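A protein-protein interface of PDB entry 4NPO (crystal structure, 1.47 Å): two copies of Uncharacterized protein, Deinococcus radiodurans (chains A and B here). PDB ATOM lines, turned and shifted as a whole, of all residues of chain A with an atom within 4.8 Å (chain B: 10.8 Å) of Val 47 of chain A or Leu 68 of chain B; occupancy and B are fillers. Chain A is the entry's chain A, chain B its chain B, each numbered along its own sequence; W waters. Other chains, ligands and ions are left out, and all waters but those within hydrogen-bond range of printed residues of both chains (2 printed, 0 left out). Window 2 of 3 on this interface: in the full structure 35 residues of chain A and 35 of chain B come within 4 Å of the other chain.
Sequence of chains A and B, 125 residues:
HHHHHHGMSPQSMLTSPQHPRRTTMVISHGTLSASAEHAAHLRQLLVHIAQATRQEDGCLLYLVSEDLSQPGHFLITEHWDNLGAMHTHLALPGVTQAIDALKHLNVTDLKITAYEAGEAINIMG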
ATOM      1  N   ARG A  43      13.204 -30.577  19.615  1.00  0.00           N
ATOM      2  CA  ARG A  43      12.195 -29.582  19.356  1.00  0.00           C
ATOM      3  C   ARG A  43      11.460 -29.932  18.073  1.00  0.00           C
ATOM      4  O   ARG A  43      10.232 -29.857  18.003  1.00  0.00           O
ATOM      5  CB  ARG A  43      12.779 -28.175  19.240  1.00  0.00           C
ATOM      6  CG  ARG A  43      13.389 -27.638  20.488  1.00  0.00           C
ATOM      7  CD  ARG A  43      13.926 -26.205  20.313  1.00  0.00           C
ATOM      8  NE  ARG A  43      14.595 -25.850  21.547  1.00  0.00           N
ATOM      9  CZ  ARG A  43      15.890 -25.945  21.789  1.00  0.00           C
ATOM     10  NH1 ARG A  43      16.730 -26.233  20.783  1.00  0.00           N
ATOM     11  NH2 ARG A  43      16.338 -25.819  23.027  1.00  0.00           N
ATOM     12  N   GLN A  44      12.219 -30.279  17.024  1.00  0.00           N
ATOM     13  CA  GLN A  44      11.617 -30.635  15.765  1.00  0.00           C
ATOM     14  C   GLN A  44      10.720 -31.881  15.851  1.00  0.00           C
ATOM     15  O   GLN A  44       9.616 -31.873  15.337  1.00  0.00           O
ATOM     16  CB  GLN A  44      12.777 -30.826  14.738  1.00  0.00           C
ATOM     17  CG  GLN A  44      13.604 -29.553  14.408  1.00  0.00           C
ATOM     18  CD  GLN A  44      15.054 -29.803  13.931  1.00  0.00           C
ATOM     19  OE1 GLN A  44      16.004 -29.024  14.231  1.00  0.00           O
ATOM     20  NE2 GLN A  44      15.240 -30.873  13.187  1.00  0.00           N
ATOM     21  N   LEU A  45      11.177 -32.896  16.565  1.00  0.00           N
ATOM     22  CA  LEU A  45      10.400 -34.092  16.717  1.00  0.00           C
ATOM     23  C   LEU A  45       9.101 -33.795  17.486  1.00  0.00           C
ATOM     24  O   LEU A  45       8.019 -34.252  17.152  1.00  0.00           O
ATOM     25  CB  LEU A  45      11.225 -35.112  17.486  1.00  0.00           C
ATOM     26  CG  LEU A  45      10.520 -36.395  17.794  1.00  0.00           C
ATOM     27  CD1 LEU A  45      10.027 -37.172  16.596  1.00  0.00           C
ATOM     28  CD2 LEU A  45      11.442 -37.264  18.630  1.00  0.00           C
ATOM     29  N   LEU A  46       9.210 -32.992  18.536  1.00  0.00           N
ATOM     30  CA  LEU A  46       8.005 -32.647  19.279  1.00  0.00           C
ATOM     31  C   LEU A  46       6.995 -31.902  18.445  1.00  0.00           C
ATOM     32  O   LEU A  46       5.820 -32.162  18.551  1.00  0.00           O
ATOM     33  CB  LEU A  46       8.375 -31.842  20.539  1.00  0.00           C
ATOM     34  CG  LEU A  46       9.044 -32.629  21.644  1.00  0.00           C
ATOM     35  CD1 LEU A  46       9.628 -31.759  22.708  1.00  0.00           C
ATOM     36  CD2 LEU A  46       8.166 -33.704  22.260  1.00  0.00           C
ATOM     37  N   VAL A  47       7.449 -30.910  17.678  1.00  0.00           N
ATOM     38  CA  VAL A  47       6.567 -30.208  16.773  1.00  0.00           C
ATOM     39  C   VAL A  47       5.874 -31.164  15.806  1.00  0.00           C
ATOM     40  O   VAL A  47       4.677 -31.086  15.618  1.00  0.00           O
ATOM     41  CB  VAL A  47       7.353 -29.120  16.050  1.00  0.00           C
ATOM     42  CG1 VAL A  47       6.541 -28.595  14.870  1.00  0.00           C
ATOM     43  CG2 VAL A  47       7.659 -28.000  17.030  1.00  0.00           C
ATOM     44  N   HIS A  48       6.629 -32.096  15.275  1.00  0.00           N
ATOM     45  CA  HIS A  48       6.039 -33.105  14.372  1.00  0.00           C
ATOM     46  C   HIS A  48       5.031 -33.971  15.072  1.00  0.00           C
ATOM     47  O   HIS A  48       3.928 -34.178  14.558  1.00  0.00           O
ATOM     48  CB  HIS A  48       7.167 -33.940  13.809  1.00  0.00           C
ATOM     49  CG  HIS A  48       7.879 -33.338  12.633  1.00  0.00           C
ATOM     50  ND1 HIS A  48       7.272 -32.530  11.692  1.00  0.00           N
ATOM     51  CD2 HIS A  48       9.193 -33.354  12.316  1.00  0.00           C
ATOM     52  CE1 HIS A  48       8.177 -32.121  10.817  1.00  0.00           C
ATOM     53  NE2 HIS A  48       9.352 -32.603  11.178  1.00  0.00           N
ATOM     54  N   ILE A  49       5.342 -34.416  16.271  1.00  0.00           N
ATOM     55  CA  ILE A  49       4.377 -35.228  16.986  1.00  0.00           C
ATOM     56  C   ILE A  49       3.084 -34.467  17.242  1.00  0.00           C
ATOM     57  O   ILE A  49       1.952 -34.983  17.099  1.00  0.00           O
ATOM     58  CB  ILE A  49       5.007 -35.737  18.297  1.00  0.00           C
ATOM     59  CG1 ILE A  49       6.109 -36.735  18.019  1.00  0.00           C
ATOM     60  CG2 ILE A  49       3.991 -36.315  19.254  1.00  0.00           C
ATOM     61  CD1 ILE A  49       7.083 -36.948  19.145  1.00  0.00           C
ATOM     62  N   ALA A  50       3.200 -33.207  17.671  1.00  0.00           N
ATOM     63  CA  ALA A  50       2.017 -32.418  17.921  1.00  0.00           C
ATOM     64  C   ALA A  50       1.140 -32.218  16.672  1.00  0.00           C
ATOM     65  O   ALA A  50      -0.055 -32.298  16.770  1.00  0.00           O
ATOM     66  CB  ALA A  50       2.412 -31.062  18.463  1.00  0.00           C
ATOM     67  N   GLN A  51       1.795 -31.945  15.556  1.00  0.00           N
ATOM     68  CA  GLN A  51       1.088 -31.678  14.263  1.00  0.00           C
ATOM     69  C   GLN A  51       0.280 -32.910  13.965  1.00  0.00           C
ATOM     70  O   GLN A  51      -0.892 -32.810  13.598  1.00  0.00           O
ATOM     71  CB  GLN A  51       2.084 -31.504  13.137  1.00  0.00           C
ATOM     72  CG  GLN A  51       2.875 -30.238  13.151  1.00  0.00           C
ATOM     73  CD  GLN A  51       4.039 -30.230  12.147  1.00  0.00           C
ATOM     74  OE1 GLN A  51       4.544 -31.263  11.702  1.00  0.00           O
ATOM     75  NE2 GLN A  51       4.466 -29.047  11.796  1.00  0.00           N
ATOM     76  N   VAL A  64       3.232 -28.651  22.585  1.00  0.00           N
ATOM     77  CA  VAL A  64       4.582 -28.943  23.002  1.00  0.00           C
ATOM     78  C   VAL A  64       5.280 -27.615  23.258  1.00  0.00           C
ATOM     79  O   VAL A  64       5.188 -26.694  22.452  1.00  0.00           O
ATOM     80  CB  VAL A  64       5.364 -29.802  22.002  1.00  0.00           C
ATOM     81  CG1 VAL A  64       4.763 -31.218  22.012  1.00  0.00           C
ATOM     82  CG2 VAL A  64       5.321 -29.287  20.569  1.00  0.00           C
ATOM     83  N   SER A  65       5.933 -27.507  24.389  1.00  0.00           N
ATOM     84  CA  SER A  65       6.492 -26.227  24.805  1.00  0.00           C
ATOM     85  C   SER A  65       7.798 -26.430  25.514  1.00  0.00           C
ATOM     86  O   SER A  65       8.146 -27.515  25.952  1.00  0.00           O
ATOM     87  CB  SER A  65       5.465 -25.439  25.592  1.00  0.00           C
ATOM     88  OG  SER A  65       5.173 -26.103  26.820  1.00  0.00           O
ATOM     89  N   GLU A  66       8.569 -25.334  25.640  1.00  0.00           N
ATOM     90  CA  GLU A  66       9.876 -25.348  26.319  1.00  0.00           C
ATOM     91  C   GLU A  66       9.842 -24.453  27.498  1.00  0.00           C
ATOM     92  O   GLU A  66       9.357 -23.316  27.412  1.00  0.00           O
ATOM     93  CB  GLU A  66      10.962 -24.935  25.317  1.00  0.00           C
ATOM     94  CG  GLU A  66      12.358 -25.069  25.870  1.00  0.00           C
ATOM     95  CD  GLU A  66      13.420 -25.015  24.832  1.00  0.00           C
ATOM     96  OE1 GLU A  66      13.100 -24.793  23.637  1.00  0.00           O
ATOM     97  OE2 GLU A  66      14.603 -25.172  25.257  1.00  0.00           O
ATOM     98  N   PHE A  74      11.277 -29.750  28.277  1.00  0.00           N
ATOM     99  CA  PHE A  74      10.086 -29.636  27.470  1.00  0.00           C
ATOM    100  C   PHE A  74       8.854 -30.162  28.173  1.00  0.00           C
ATOM    101  O   PHE A  74       8.947 -30.972  29.115  1.00  0.00           O
ATOM    102  CB  PHE A  74      10.280 -30.367  26.177  1.00  0.00           C
ATOM    103  CG  PHE A  74      11.455 -29.862  25.401  1.00  0.00           C
ATOM    104  CD1 PHE A  74      11.300 -28.691  24.673  1.00  0.00           C
ATOM    105  CD2 PHE A  74      12.698 -30.441  25.437  1.00  0.00           C
ATOM    106  CE1 PHE A  74      12.367 -28.140  24.020  1.00  0.00           C
ATOM    107  CE2 PHE A  74      13.730 -29.918  24.765  1.00  0.00           C
ATOM    108  CZ  PHE A  74      13.579 -28.743  24.036  1.00  0.00           C
ATOM    109  N   LEU B  32      -1.379 -17.378  26.711  1.00  0.00           N
ATOM    110  CA  LEU B  32      -1.300 -15.965  26.412  1.00  0.00           C
ATOM    111  C   LEU B  32      -0.303 -15.779  25.315  1.00  0.00           C
ATOM    112  O   LEU B  32       0.525 -16.660  25.108  1.00  0.00           O
ATOM    113  CB  LEU B  32      -0.943 -15.160  27.634  1.00  0.00           C
ATOM    114  CG  LEU B  32       0.450 -15.384  28.258  1.00  0.00           C
ATOM    115  CD1 LEU B  32       0.791 -14.214  29.142  1.00  0.00           C
ATOM    116  CD2 LEU B  32       0.570 -16.680  29.063  1.00  0.00           C
ATOM    117  N   ARG B  43       8.759 -12.958  28.437  1.00  0.00           N
ATOM    118  CA  ARG B  43       9.448 -14.124  28.864  1.00  0.00           C
ATOM    119  C   ARG B  43      10.053 -13.926  30.228  1.00  0.00           C
ATOM    120  O   ARG B  43       9.950 -14.761  31.076  1.00  0.00           O
ATOM    121  CB  ARG B  43      10.506 -14.560  27.857  1.00  0.00           C
ATOM    122  CG  ARG B  43       9.994 -14.959  26.496  1.00  0.00           C
ATOM    123  CD  ARG B  43      11.099 -15.396  25.518  1.00  0.00           C
ATOM    124  NE  ARG B  43      10.543 -15.706  24.235  1.00  0.00           N
ATOM    125  CZ  ARG B  43      10.372 -14.862  23.233  1.00  0.00           C
ATOM    126  NH1 ARG B  43      10.937 -13.662  23.273  1.00  0.00           N
ATOM    127  NH2 ARG B  43       9.662 -15.171  22.189  1.00  0.00           N
ATOM    128  N   VAL B  64       6.276 -22.055  33.354  1.00  0.00           N
ATOM    129  CA  VAL B  64       6.020 -21.146  32.277  1.00  0.00           C
ATOM    130  C   VAL B  64       6.808 -21.619  31.093  1.00  0.00           C
ATOM    131  O   VAL B  64       7.997 -21.898  31.184  1.00  0.00           O
ATOM    132  CB  VAL B  64       6.291 -19.695  32.650  1.00  0.00           C
ATOM    133  CG1 VAL B  64       5.233 -19.203  33.641  1.00  0.00           C
ATOM    134  CG2 VAL B  64       7.736 -19.488  33.132  1.00  0.00           C
ATOM    135  N   SER B  65       6.130 -21.741  29.955  1.00  0.00           N
ATOM    136  CA  SER B  65       6.783 -22.283  28.778  1.00  0.00           C
ATOM    137  C   SER B  65       6.321 -21.601  27.528  1.00  0.00           C
ATOM    138  O   SER B  65       5.339 -20.895  27.538  1.00  0.00           O
ATOM    139  CB  SER B  65       6.550 -23.784  28.719  1.00  0.00           C
ATOM    140  OG  SER B  65       5.179 -24.106  28.542  1.00  0.00           O
ATOM    141  N   GLU B  66       7.056 -21.811  26.441  1.00  0.00           N
ATOM    142  CA  GLU B  66       6.759 -21.214  25.167  1.00  0.00           C
ATOM    143  C   GLU B  66       6.471 -22.304  24.155  1.00  0.00           C
ATOM    144  O   GLU B  66       7.231 -23.266  24.011  1.00  0.00           O
ATOM    145  CB  GLU B  66       7.844 -20.264  24.715  1.00  0.00           C
ATOM    146  CG  GLU B  66       7.482 -19.454  23.498  1.00  0.00           C
ATOM    147  CD  GLU B  66       8.482 -18.371  23.202  1.00  0.00           C
ATOM    148  OE1 GLU B  66       9.492 -18.282  23.887  1.00  0.00           O
ATOM    149  OE2 GLU B  66       8.229 -17.647  22.200  1.00  0.00           O
ATOM    150  N   ASP B  67       5.369 -22.155  23.442  1.00  0.00           N
ATOM    151  CA  ASP B  67       4.876 -23.100  22.468  1.00  0.00           C
ATOM    152  C   ASP B  67       5.893 -23.275  21.364  1.00  0.00           C
ATOM    153  O   ASP B  67       6.127 -22.319  20.591  1.00  0.00           O
ATOM    154  CB  ASP B  67       3.560 -22.575  21.908  1.00  0.00           C
ATOM    155  CG  ASP B  67       2.833 -23.538  21.029  1.00  0.00           C
ATOM    156  OD1 ASP B  67       3.433 -24.522  20.541  1.00  0.00           O
ATOM    157  OD2 ASP B  67       1.605 -23.293  20.839  1.00  0.00           O
ATOM    158  N   LEU B  68       6.435 -24.474  21.209  1.00  0.00           N
ATOM    159  CA  LEU B  68       7.416 -24.766  20.168  1.00  0.00           C
ATOM    160  C   LEU B  68       6.855 -24.588  18.764  1.00  0.00           C
ATOM    161  O   LEU B  68       7.597 -24.338  17.791  1.00  0.00           O
ATOM    162  CB  LEU B  68       7.966 -26.167  20.308  1.00  0.00           C
ATOM    163  CG  LEU B  68       8.854 -26.450  21.473  1.00  0.00           C
ATOM    164  CD1 LEU B  68       9.139 -27.943  21.583  1.00  0.00           C
ATOM    165  CD2 LEU B  68      10.111 -25.640  21.373  1.00  0.00           C
ATOM    166  N   SER B  69       5.554 -24.689  18.638  1.00  0.00           N
ATOM    167  CA  SER B  69       4.864 -24.567  17.327  1.00  0.00           C
ATOM    168  C   SER B  69       4.491 -23.117  17.065  1.00  0.00           C
ATOM    169  O   SER B  69       4.062 -22.808  15.923  1.00  0.00           O
ATOM    170  CB  SER B  69       3.577 -25.400  17.353  1.00  0.00           C
ATOM    171  OG  SER B  69       3.885 -26.785  17.629  1.00  0.00           O
ATOM    172  N   GLN B  70       4.567 -22.243  18.038  1.00  0.00           N
ATOM    173  CA  GLN B  70       4.032 -20.917  17.919  1.00  0.00           C
ATOM    174  C   GLN B  70       4.842 -19.977  18.800  1.00  0.00           C
ATOM    175  O   GLN B  70       4.455 -19.633  19.896  1.00  0.00           O
ATOM    176  CB  GLN B  70       2.589 -20.850  18.333  1.00  0.00           C
ATOM    177  CG  GLN B  70       1.570 -21.463  17.492  1.00  0.00           C
ATOM    178  CD  GLN B  70       0.298 -20.716  17.757  1.00  0.00           C
ATOM    179  OE1 GLN B  70      -0.180 -19.950  16.937  1.00  0.00           O
ATOM    180  NE2 GLN B  70      -0.167 -20.836  18.938  1.00  0.00           N
ATOM    181  N   PRO B  71       5.999 -19.516  18.314  1.00  0.00           N
ATOM    182  CA  PRO B  71       6.757 -18.562  19.044  1.00  0.00           C
ATOM    183  C   PRO B  71       5.878 -17.353  19.441  1.00  0.00           C
ATOM    184  O   PRO B  71       5.024 -16.964  18.635  1.00  0.00           O
ATOM    185  CB  PRO B  71       7.862 -18.174  18.076  1.00  0.00           C
ATOM    186  CG  PRO B  71       8.055 -19.340  17.216  1.00  0.00           C
ATOM    187  CD  PRO B  71       6.674 -19.907  17.051  1.00  0.00           C
ATOM    188  N   GLY B  72       6.071 -16.840  20.632  1.00  0.00           N
ATOM    189  CA  GLY B  72       5.277 -15.773  21.130  1.00  0.00           C
ATOM    190  C   GLY B  72       4.020 -16.187  21.806  1.00  0.00           C
ATOM    191  O   GLY B  72       3.304 -15.298  22.341  1.00  0.00           O
ATOM    192  N   HIS B  73       3.765 -17.485  21.850  1.00  0.00           N
ATOM    193  CA  HIS B  73       2.627 -17.996  22.534  1.00  0.00           C
ATOM    194  C   HIS B  73       3.093 -18.863  23.693  1.00  0.00           C
ATOM    195  O   HIS B  73       3.973 -19.707  23.555  1.00  0.00           O
ATOM    196  CB  HIS B  73       1.789 -18.685  21.527  1.00  0.00           C
ATOM    197  CG  HIS B  73       1.366 -17.756  20.434  1.00  0.00           C
ATOM    198  ND1 HIS B  73       2.251 -17.154  19.562  1.00  0.00           N
ATOM    199  CD2 HIS B  73       0.144 -17.285  20.121  1.00  0.00           C
ATOM    200  CE1 HIS B  73       1.580 -16.343  18.761  1.00  0.00           C
ATOM    201  NE2 HIS B  73       0.301 -16.407  19.088  1.00  0.00           N
ATOM    202  N   PHE B  74       2.574 -18.514  24.862  1.00  0.00           N
ATOM    203  CA  PHE B  74       3.081 -19.008  26.123  1.00  0.00           C
ATOM    204  C   PHE B  74       2.012 -19.795  26.841  1.00  0.00           C
ATOM    205  O   PHE B  74       0.787 -19.607  26.687  1.00  0.00           O
ATOM    206  CB  PHE B  74       3.544 -17.824  26.961  1.00  0.00           C
ATOM    207  CG  PHE B  74       4.647 -17.051  26.317  1.00  0.00           C
ATOM    208  CD1 PHE B  74       5.919 -17.518  26.361  1.00  0.00           C
ATOM    209  CD2 PHE B  74       4.379 -15.960  25.541  1.00  0.00           C
ATOM    210  CE1 PHE B  74       6.969 -16.864  25.713  1.00  0.00           C
ATOM    211  CE2 PHE B  74       5.401 -15.308  24.873  1.00  0.00           C
ATOM    212  CZ  PHE B  74       6.693 -15.782  24.968  1.00  0.00           C
ATOM    213  N   LEU B  75       2.537 -20.670  27.699  1.00  0.00           N
ATOM    214  CA  LEU B  75       1.723 -21.521  28.545  1.00  0.00           C
ATOM    215  C   LEU B  75       2.100 -21.314  29.983  1.00  0.00           C
ATOM    216  O   LEU B  75       3.279 -21.195  30.332  1.00  0.00           O
ATOM    217  CB  LEU B  75       1.932 -22.971  28.183  1.00  0.00           C
ATOM    218  CG  LEU B  75       1.329 -23.571  26.972  1.00  0.00           C
ATOM    219  CD1 LEU B  75       1.980 -22.994  25.765  1.00  0.00           C
ATOM    220  CD2 LEU B  75       1.480 -25.073  27.001  1.00  0.00           C
HETATM  221  O   HOH W   1       3.244 -28.525  15.674  1.00  0.00           O
HETATM  222  O   HOH W   2       2.699 -27.084  20.190  1.00  0.00           O
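Water W2 lies within hydrogen-bond range of OD1 of Asp 67 of chain B, OG of Ser 69 of chain B and N of Val 64 of chain A. Water W1 bridges OG of Ser 69 of chain B (2.7 Å) and O of Val 47 of chain A (2.9 Å).
The side-chain hydroxyl of Ser 65 of chain A is in hydrogen-bond range of the side-chain hydroxyl of Ser 65 of chain B, at 2.6 Å. The backbone NH (N) of Glu 66 of chain B sits at hydrogen-bond distance from the backbone carbonyl oxygen (O) of Glu 66 of chain A, 2.9 Å away. The backbone carbonyl oxygen of Val 64 of chain A is in hydrogen-bond range of the backbone NH of Leu 68 of chain B, 2.8 Å away. The backbone carbonyl oxygen (O) of Val 64 of chain A sits close to the side-chain carboxylate (OD1) of Asp 67 of chain B, 3.4 Å away.
Ser 65 of chain A touches its own counterpart, Ser 65 of chain B. Ser 65 of chain A touches Glu 66 of chain B, and with the chains exchanged Glu 66 of chain A touches Ser 65 of chain B. Glu 66 of chain B touches its own counterpart, Glu 66 of chain A. Positions printed for both chains: 43, 64, 65, 66 and 74. Of the 12 pairs that touch across the chains among the printed residues, 4 have their exchanged pair printed and touching as well.
Arg 43 of chain A touches Leu 68 of chain B (CG to CD2, 3.9 Å). CG2 of Val 47 of chain A touches O of Leu 68 of chain B (3.7 Å). CA of Ser 65 of chain A touches O of Glu 66 of chain B (3.2 Å). CB of Ser 65 of chain A touches N of Asp 67 of chain B, 3.9 Å away. Leu 75 of chain B touches Ser 65 of chain A. O of Glu 66 of chain A touches CA of Ser 65 of chain B, at 3.1 Å. CD2 of Leu 68 of chain B touches OE1 of Glu 66 of chain A, 3.8 Å away. CD1 of Phe 74 of chain A touches CD1 of Leu 68 of chain B, at 3.8 Å.
Of the 14 printed residues of chain B, 5 touch a printed residue of chain A. Printed residues of chain B that touch a printed residue of chain A: Ser 65, Glu 66, Asp 67, Leu 68 and Leu 75. Hydrophobic or aromatic side chains of chain B within 4 Å of the printed part of chain A: Leu 68 and Leu 75. Hydrophobic or aromatic side chains of chain A that line the printed part of chain B: Val 47 and Phe 74. Among the printed residues, no Asp or Glu carboxylate lies within 4 Å of a Lys or Arg side-chain nitrogen of the other chain.
The backbone NH of Asp 67 of chain B sits at hydrogen-bond distance from the backbone carbonyl oxygen of His 73 of chain B, at 2.8 Å. The guanidinium group (NE) of Arg 43 of chain B lies within salt-bridge range of the side-chain carboxylate (OE1) of Glu 66 of chain B, 2.8 Å away. NE of Arg 43 of chain A is in salt-bridge range of OE1 of Glu 66 of chain A. The backbone NH (N) of Ser 69 of chain B is in hydrogen-bond range of the side-chain carboxylate (OD1) of Asp 67 of chain B, 2.9 Å away. O of Ser 65 of chain B lies within hydrogen-bond range of N of Leu 75 of chain B. N of Gly 72 of chain B is in hydrogen-bond range of OE2 of Glu 66 of chain B (2.8 Å).
Printed residues of chain B within 4 Å of Val 47 of chain A: Leu 68. Of the printed residues of chain A, Leu 68 of chain B touches Arg 43, Val 47, Val 64, Glu 66 and Phe 74. Arg 43 of chain A touches one residue of chain B. No residue of chain B comes within 4 Å of Ile 49 of chain A. No residue of chain B comes within 4 Å of Ala 50 of chain A. Val 64 of chain A touches just these residues of chain B: Asp 67 (3.4 Å) and Leu 68 (2.8 Å). Of chain B, only Ser 65 (3.1 Å), Glu 66 (2.9 Å) and Leu 68 (3.8 Å) come within 4 Å of Glu 66 of chain A. Of the printed residues of chain A, Ser 65 of chain B touches Ser 65 and Glu 66. Of the printed residues of chain A, Asp 67 of chain B touches Val 64 (3.4 Å) and Ser 65 (3.9 Å). Of the printed residues of chain B, Phe 74 of chain A touches Leu 68 (3.8 Å). Of the printed residues of chain A, Leu 75 of chain B touches Ser 65. Of the printed residues of chain A, Glu 66 of chain B touches Ser 65 and Glu 66. The nearest printed residue of chain A that does not touch Leu 68 of chain B is Ser 65 of chain A (4.001 Å).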
